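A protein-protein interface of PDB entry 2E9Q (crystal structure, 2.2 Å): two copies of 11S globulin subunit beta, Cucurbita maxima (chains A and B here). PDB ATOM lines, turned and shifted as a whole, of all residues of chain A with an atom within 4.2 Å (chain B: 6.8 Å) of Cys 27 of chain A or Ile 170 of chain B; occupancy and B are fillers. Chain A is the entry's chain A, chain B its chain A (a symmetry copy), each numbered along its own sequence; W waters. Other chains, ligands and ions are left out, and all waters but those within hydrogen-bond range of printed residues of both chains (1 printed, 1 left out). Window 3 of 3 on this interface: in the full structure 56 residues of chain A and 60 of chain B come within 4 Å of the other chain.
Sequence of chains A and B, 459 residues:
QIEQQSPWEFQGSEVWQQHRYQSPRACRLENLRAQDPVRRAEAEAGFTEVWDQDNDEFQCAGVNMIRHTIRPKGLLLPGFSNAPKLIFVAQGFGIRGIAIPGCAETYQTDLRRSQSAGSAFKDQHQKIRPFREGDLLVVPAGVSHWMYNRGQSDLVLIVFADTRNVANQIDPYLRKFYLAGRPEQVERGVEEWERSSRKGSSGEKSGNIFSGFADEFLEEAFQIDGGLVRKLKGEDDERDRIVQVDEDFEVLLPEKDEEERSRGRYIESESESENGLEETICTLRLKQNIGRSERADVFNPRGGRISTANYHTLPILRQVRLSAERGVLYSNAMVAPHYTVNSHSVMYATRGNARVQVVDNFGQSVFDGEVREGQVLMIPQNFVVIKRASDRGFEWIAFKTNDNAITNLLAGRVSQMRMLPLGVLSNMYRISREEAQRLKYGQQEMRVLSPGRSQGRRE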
ATOM      1  N   ALA A  26       6.542   2.220  -8.174  1.00  0.00           N
ATOM      2  CA  ALA A  26       6.506   1.944  -6.710  1.00  0.00           C
ATOM      3  C   ALA A  26       7.883   2.090  -6.071  1.00  0.00           C
ATOM      4  O   ALA A  26       8.909   1.771  -6.683  1.00  0.00           O
ATOM      5  CB  ALA A  26       5.970   0.539  -6.452  1.00  0.00           C
ATOM      6  N   CYS A  27       7.893   2.575  -4.835  1.00  0.00           N
ATOM      7  CA  CYS A  27       9.122   2.759  -4.076  1.00  0.00           C
ATOM      8  C   CYS A  27       9.487   1.449  -3.378  1.00  0.00           C
ATOM      9  O   CYS A  27       8.626   0.802  -2.801  1.00  0.00           O
ATOM     10  CB  CYS A  27       8.906   3.843  -3.023  1.00  0.00           C
ATOM     11  SG  CYS A  27       8.961   5.562  -3.623  1.00  0.00           S
ATOM     12  N   ARG A  28      10.755   1.053  -3.442  1.00  0.00           N
ATOM     13  CA  ARG A  28      11.201  -0.173  -2.771  1.00  0.00           C
ATOM     14  C   ARG A  28      11.726   0.206  -1.388  1.00  0.00           C
ATOM     15  O   ARG A  28      12.901   0.529  -1.227  1.00  0.00           O
ATOM     16  CB  ARG A  28      12.310  -0.866  -3.567  1.00  0.00           C
ATOM     17  CG  ARG A  28      11.834  -1.551  -4.830  1.00  0.00           C
ATOM     18  CD  ARG A  28      12.709  -2.761  -5.166  1.00  0.00           C
ATOM     19  NE  ARG A  28      14.088  -2.398  -5.493  1.00  0.00           N
ATOM     20  CZ  ARG A  28      15.023  -3.268  -5.873  1.00  0.00           C
ATOM     21  NH1 ARG A  28      14.730  -4.559  -5.971  1.00  0.00           N
ATOM     22  NH2 ARG A  28      16.247  -2.846  -6.165  1.00  0.00           N
ATOM     23  N   LEU A  29      10.842   0.158  -0.401  1.00  0.00           N
ATOM     24  CA  LEU A  29      11.181   0.544   0.960  1.00  0.00           C
ATOM     25  C   LEU A  29      11.064  -0.584   1.968  1.00  0.00           C
ATOM     26  O   LEU A  29      10.632  -0.361   3.100  1.00  0.00           O
ATOM     27  CB  LEU A  29      10.264   1.674   1.394  1.00  0.00           C
ATOM     28  CG  LEU A  29      10.135   2.832   0.412  1.00  0.00           C
ATOM     29  CD1 LEU A  29       9.048   3.783   0.900  1.00  0.00           C
ATOM     30  CD2 LEU A  29      11.482   3.536   0.291  1.00  0.00           C
ATOM     31  N   CYS A  60      13.561   6.871  -4.050  1.00  0.00           N
ATOM     32  CA  CYS A  60      12.167   7.139  -3.733  1.00  0.00           C
ATOM     33  C   CYS A  60      12.005   8.599  -3.344  1.00  0.00           C
ATOM     34  O   CYS A  60      11.143   9.313  -3.875  1.00  0.00           O
ATOM     35  CB  CYS A  60      11.715   6.264  -2.578  1.00  0.00           C
ATOM     36  SG  CYS A  60       9.973   6.504  -2.122  1.00  0.00           S
ATOM     37  N   GLN A 381       8.885   8.988   4.972  1.00  0.00           N
ATOM     38  CA  GLN A 381       7.754   9.667   5.560  1.00  0.00           C
ATOM     39  C   GLN A 381       6.783   8.625   6.130  1.00  0.00           C
ATOM     40  O   GLN A 381       6.475   7.616   5.472  1.00  0.00           O
ATOM     41  CB  GLN A 381       7.051  10.495   4.473  1.00  0.00           C
ATOM     42  CG  GLN A 381       5.784  11.219   4.929  1.00  0.00           C
ATOM     43  CD  GLN A 381       4.940  11.728   3.762  1.00  0.00           C
ATOM     44  OE1 GLN A 381       3.926  12.389   3.967  1.00  0.00           O
ATOM     45  NE2 GLN A 381       5.356  11.410   2.536  1.00  0.00           N
ATOM     46  N   ASN B  82      -0.477   7.721   4.404  1.00  0.00           N
ATOM     47  CA  ASN B  82       0.366   8.636   3.643  1.00  0.00           C
ATOM     48  C   ASN B  82      -0.408   9.552   2.713  1.00  0.00           C
ATOM     49  O   ASN B  82       0.176  10.396   2.055  1.00  0.00           O
ATOM     50  CB  ASN B  82       1.388   7.835   2.832  1.00  0.00           C
ATOM     51  CG  ASN B  82       0.735   6.927   1.790  1.00  0.00           C
ATOM     52  OD1 ASN B  82      -0.357   6.396   2.003  1.00  0.00           O
ATOM     53  ND2 ASN B  82       1.414   6.731   0.669  1.00  0.00           N
ATOM     54  N   ALA B 167       0.757  16.192  -0.260  1.00  0.00           N
ATOM     55  CA  ALA B 167       1.111  15.691   1.070  1.00  0.00           C
ATOM     56  C   ALA B 167       1.802  14.325   1.077  1.00  0.00           C
ATOM     57  O   ALA B 167       2.504  13.989   2.027  1.00  0.00           O
ATOM     58  CB  ALA B 167      -0.135  15.645   1.962  1.00  0.00           C
ATOM     59  N   ASN B 168       1.612  13.534   0.028  1.00  0.00           N
ATOM     60  CA  ASN B 168       2.250  12.214  -0.031  1.00  0.00           C
ATOM     61  C   ASN B 168       3.559  12.291  -0.806  1.00  0.00           C
ATOM     62  O   ASN B 168       3.561  12.563  -2.000  1.00  0.00           O
ATOM     63  CB  ASN B 168       1.291  11.202  -0.668  1.00  0.00           C
ATOM     64  CG  ASN B 168       1.955   9.883  -1.013  1.00  0.00           C
ATOM     65  OD1 ASN B 168       2.909   9.456  -0.366  1.00  0.00           O
ATOM     66  ND2 ASN B 168       1.429   9.221  -2.036  1.00  0.00           N
ATOM     67  N   GLN B 169       4.671  12.053  -0.122  1.00  0.00           N
ATOM     68  CA  GLN B 169       5.978  12.122  -0.766  1.00  0.00           C
ATOM     69  C   GLN B 169       6.577  10.754  -1.076  1.00  0.00           C
ATOM     70  O   GLN B 169       7.723  10.668  -1.514  1.00  0.00           O
ATOM     71  CB  GLN B 169       6.967  12.899   0.107  1.00  0.00           C
ATOM     72  CG  GLN B 169       6.512  14.302   0.499  1.00  0.00           C
ATOM     73  CD  GLN B 169       7.653  15.135   1.075  1.00  0.00           C
ATOM     74  OE1 GLN B 169       8.767  14.638   1.257  1.00  0.00           O
ATOM     75  NE2 GLN B 169       7.381  16.403   1.363  1.00  0.00           N
ATOM     76  N   ILE B 170       5.820   9.686  -0.840  1.00  0.00           N
ATOM     77  CA  ILE B 170       6.344   8.357  -1.110  1.00  0.00           C
ATOM     78  C   ILE B 170       6.086   7.951  -2.559  1.00  0.00           C
ATOM     79  O   ILE B 170       6.863   8.290  -3.451  1.00  0.00           O
ATOM     80  CB  ILE B 170       5.725   7.306  -0.174  1.00  0.00           C
ATOM     81  CG1 ILE B 170       5.922   7.732   1.284  1.00  0.00           C
ATOM     82  CG2 ILE B 170       6.384   5.952  -0.414  1.00  0.00           C
ATOM     83  CD1 ILE B 170       5.133   6.905   2.267  1.00  0.00           C
ATOM     84  N   ASP B 171       5.004   7.214  -2.784  1.00  0.00           N
ATOM     85  CA  ASP B 171       4.644   6.771  -4.127  1.00  0.00           C
ATOM     86  C   ASP B 171       3.122   6.731  -4.202  1.00  0.00           C
ATOM     87  O   ASP B 171       2.452   6.824  -3.177  1.00  0.00           O
ATOM     88  CB  ASP B 171       5.266   5.395  -4.422  1.00  0.00           C
ATOM     89  CG  ASP B 171       4.752   4.316  -3.508  1.00  0.00           C
ATOM     90  OD1 ASP B 171       5.407   3.252  -3.415  1.00  0.00           O
ATOM     91  OD2 ASP B 171       3.689   4.526  -2.885  1.00  0.00           O
ATOM     92  N   PRO B 172       2.559   6.570  -5.411  1.00  0.00           N
ATOM     93  CA  PRO B 172       1.110   6.531  -5.641  1.00  0.00           C
ATOM     94  C   PRO B 172       0.366   5.355  -5.037  1.00  0.00           C
ATOM     95  O   PRO B 172      -0.724   5.002  -5.487  1.00  0.00           O
ATOM     96  CB  PRO B 172       1.010   6.552  -7.159  1.00  0.00           C
ATOM     97  CG  PRO B 172       2.180   5.710  -7.546  1.00  0.00           C
ATOM     98  CD  PRO B 172       3.283   6.248  -6.654  1.00  0.00           C
ATOM     99  N   TYR B 173       0.940   4.771  -3.998  1.00  0.00           N
ATOM    100  CA  TYR B 173       0.340   3.628  -3.339  1.00  0.00           C
ATOM    101  C   TYR B 173      -0.044   3.923  -1.882  1.00  0.00           C
ATOM    102  O   TYR B 173       0.756   4.406  -1.083  1.00  0.00           O
ATOM    103  CB  TYR B 173       1.294   2.431  -3.403  1.00  0.00           C
ATOM    104  CG  TYR B 173       1.468   1.883  -4.805  1.00  0.00           C
ATOM    105  CD1 TYR B 173       0.409   1.265  -5.462  1.00  0.00           C
ATOM    106  CD2 TYR B 173       2.682   2.001  -5.480  1.00  0.00           C
ATOM    107  CE1 TYR B 173       0.548   0.777  -6.756  1.00  0.00           C
ATOM    108  CE2 TYR B 173       2.833   1.516  -6.776  1.00  0.00           C
ATOM    109  CZ  TYR B 173       1.763   0.906  -7.408  1.00  0.00           C
ATOM    110  OH  TYR B 173       1.909   0.421  -8.689  1.00  0.00           O
ATOM    111  N   ARG B 175      -0.935   3.561   1.943  1.00  0.00           N
ATOM    112  CA  ARG B 175      -0.397   2.825   3.079  1.00  0.00           C
ATOM    113  C   ARG B 175      -1.112   3.287   4.352  1.00  0.00           C
ATOM    114  O   ARG B 175      -1.223   4.484   4.608  1.00  0.00           O
ATOM    115  CB  ARG B 175       1.107   3.095   3.218  1.00  0.00           C
ATOM    116  CG  ARG B 175       1.944   2.775   1.983  1.00  0.00           C
ATOM    117  CD  ARG B 175       3.424   3.021   2.242  1.00  0.00           C
ATOM    118  NE  ARG B 175       4.288   2.521   1.172  1.00  0.00           N
ATOM    119  CZ  ARG B 175       4.287   2.979  -0.076  1.00  0.00           C
ATOM    120  NH1 ARG B 175       3.464   3.958  -0.432  1.00  0.00           N
ATOM    121  NH2 ARG B 175       5.117   2.458  -0.974  1.00  0.00           N
ATOM    122  N   PHE B 177      -1.013   2.924   8.469  1.00  0.00           N
ATOM    123  CA  PHE B 177      -0.283   2.483   9.660  1.00  0.00           C
ATOM    124  C   PHE B 177      -1.220   2.405  10.868  1.00  0.00           C
ATOM    125  O   PHE B 177      -1.649   3.436  11.401  1.00  0.00           O
ATOM    126  CB  PHE B 177       0.863   3.463   9.986  1.00  0.00           C
ATOM    127  CG  PHE B 177       1.838   3.671   8.856  1.00  0.00           C
ATOM    128  CD1 PHE B 177       1.457   4.352   7.703  1.00  0.00           C
ATOM    129  CD2 PHE B 177       3.130   3.171   8.937  1.00  0.00           C
ATOM    130  CE1 PHE B 177       2.355   4.528   6.640  1.00  0.00           C
ATOM    131  CE2 PHE B 177       4.037   3.343   7.874  1.00  0.00           C
ATOM    132  CZ  PHE B 177       3.641   4.022   6.730  1.00  0.00           C
HETATM  133  O   HOH W   1       8.732   8.532  -6.109  1.00  0.00           O
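The backbone NH (N) of Gln 169 of chain B sits close to the side-chain amide nitrogen (NE2) of Gln 381 of chain A, at 2.8 Å.
The backbone carbonyl oxygen (O) of Ala 167 of chain B sits close to the side-chain amide oxygen (OE1) of Gln 381 of chain A (2.9 Å).
O of Ile 170 of chain B sits close to SG of Cys 27 of chain A (3.4 Å).
OD1 of Asp 171 of chain B sits at hydrogen-bond distance from N of Cys 27 of chain A.
The side-chain amide oxygen of Asn 168 of chain B lies within hydrogen-bond range of the backbone NH of Ile 170 of chain B, 3.0 Å away.
The side-chain amide nitrogen (ND2) of Asn 82 of chain B lies within hydrogen-bond range of the backbone carbonyl oxygen (O) of Tyr 173 of chain B, at 3.0 Å.
ND2 of Asn 168 of chain B sits at hydrogen-bond distance from O of Asp 171 of chain B, 2.8 Å away.
SG of Cys 60 of chain A is disulfide-bonded to SG of Cys 27 of chain A (2.0 Å).
OD1 of Asn 168 of chain B sits at hydrogen-bond distance from ND2 of Asn 82 of chain B, 3.3 Å away.
The side-chain carboxylate (OD2) of Asp 171 of chain B is in salt-bridge range of the guanidinium group (NH1) of Arg 175 of chain B (2.5 Å).
Among the printed residues, merely in contact across the chains: Ala 26 of chain A with Asp 171 of chain B, Ala 26 of chain A with Tyr 173 of chain B, Leu 29 of chain A with Ile 170 of chain B, Cys 60 of chain A with Ile 170 of chain B, Gln 381 of chain A with Asn 168 of chain B and Gln 381 of chain A with Ile 170 of chain B.
Cys 27 of chain A touches just these residues of chain B: Ile 170 and Asp 171.
Ile 170 of chain B touches just these residues of chain A: Cys 27, Leu 29, Cys 60 and Gln 381.
Printed residues of chain A within 4 Å of Asn 168 of chain B: Gln 381 (3.9 Å).
Printed residues of chain A within 4 Å of Tyr 173 of chain B: Ala 26 (3.3 Å).
Printed residues of chain A within 4 Å of Gln 169 of chain B: Gln 381.
Pro 172 of chain B touches none of the printed residues of chain A.
Hydrophobic or aromatic side chains of chain A that line the printed part of chain B: Ala 26 and Leu 29.
Of the 10 printed residues of chain B, 6 touch a printed residue of chain A.
Among the printed residues, no Asp or Glu carboxylate lies within 4 Å of a Lys or Arg side-chain nitrogen of the other chain.
No position is printed for both chains.
Water W1 lies within hydrogen-bond range of the backbone carbonyl oxygen (O) of Ile 170 of chain B (3.3 Å) and the backbone carbonyl oxygen (O) of Cys 60 of chain A (3.4 Å).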
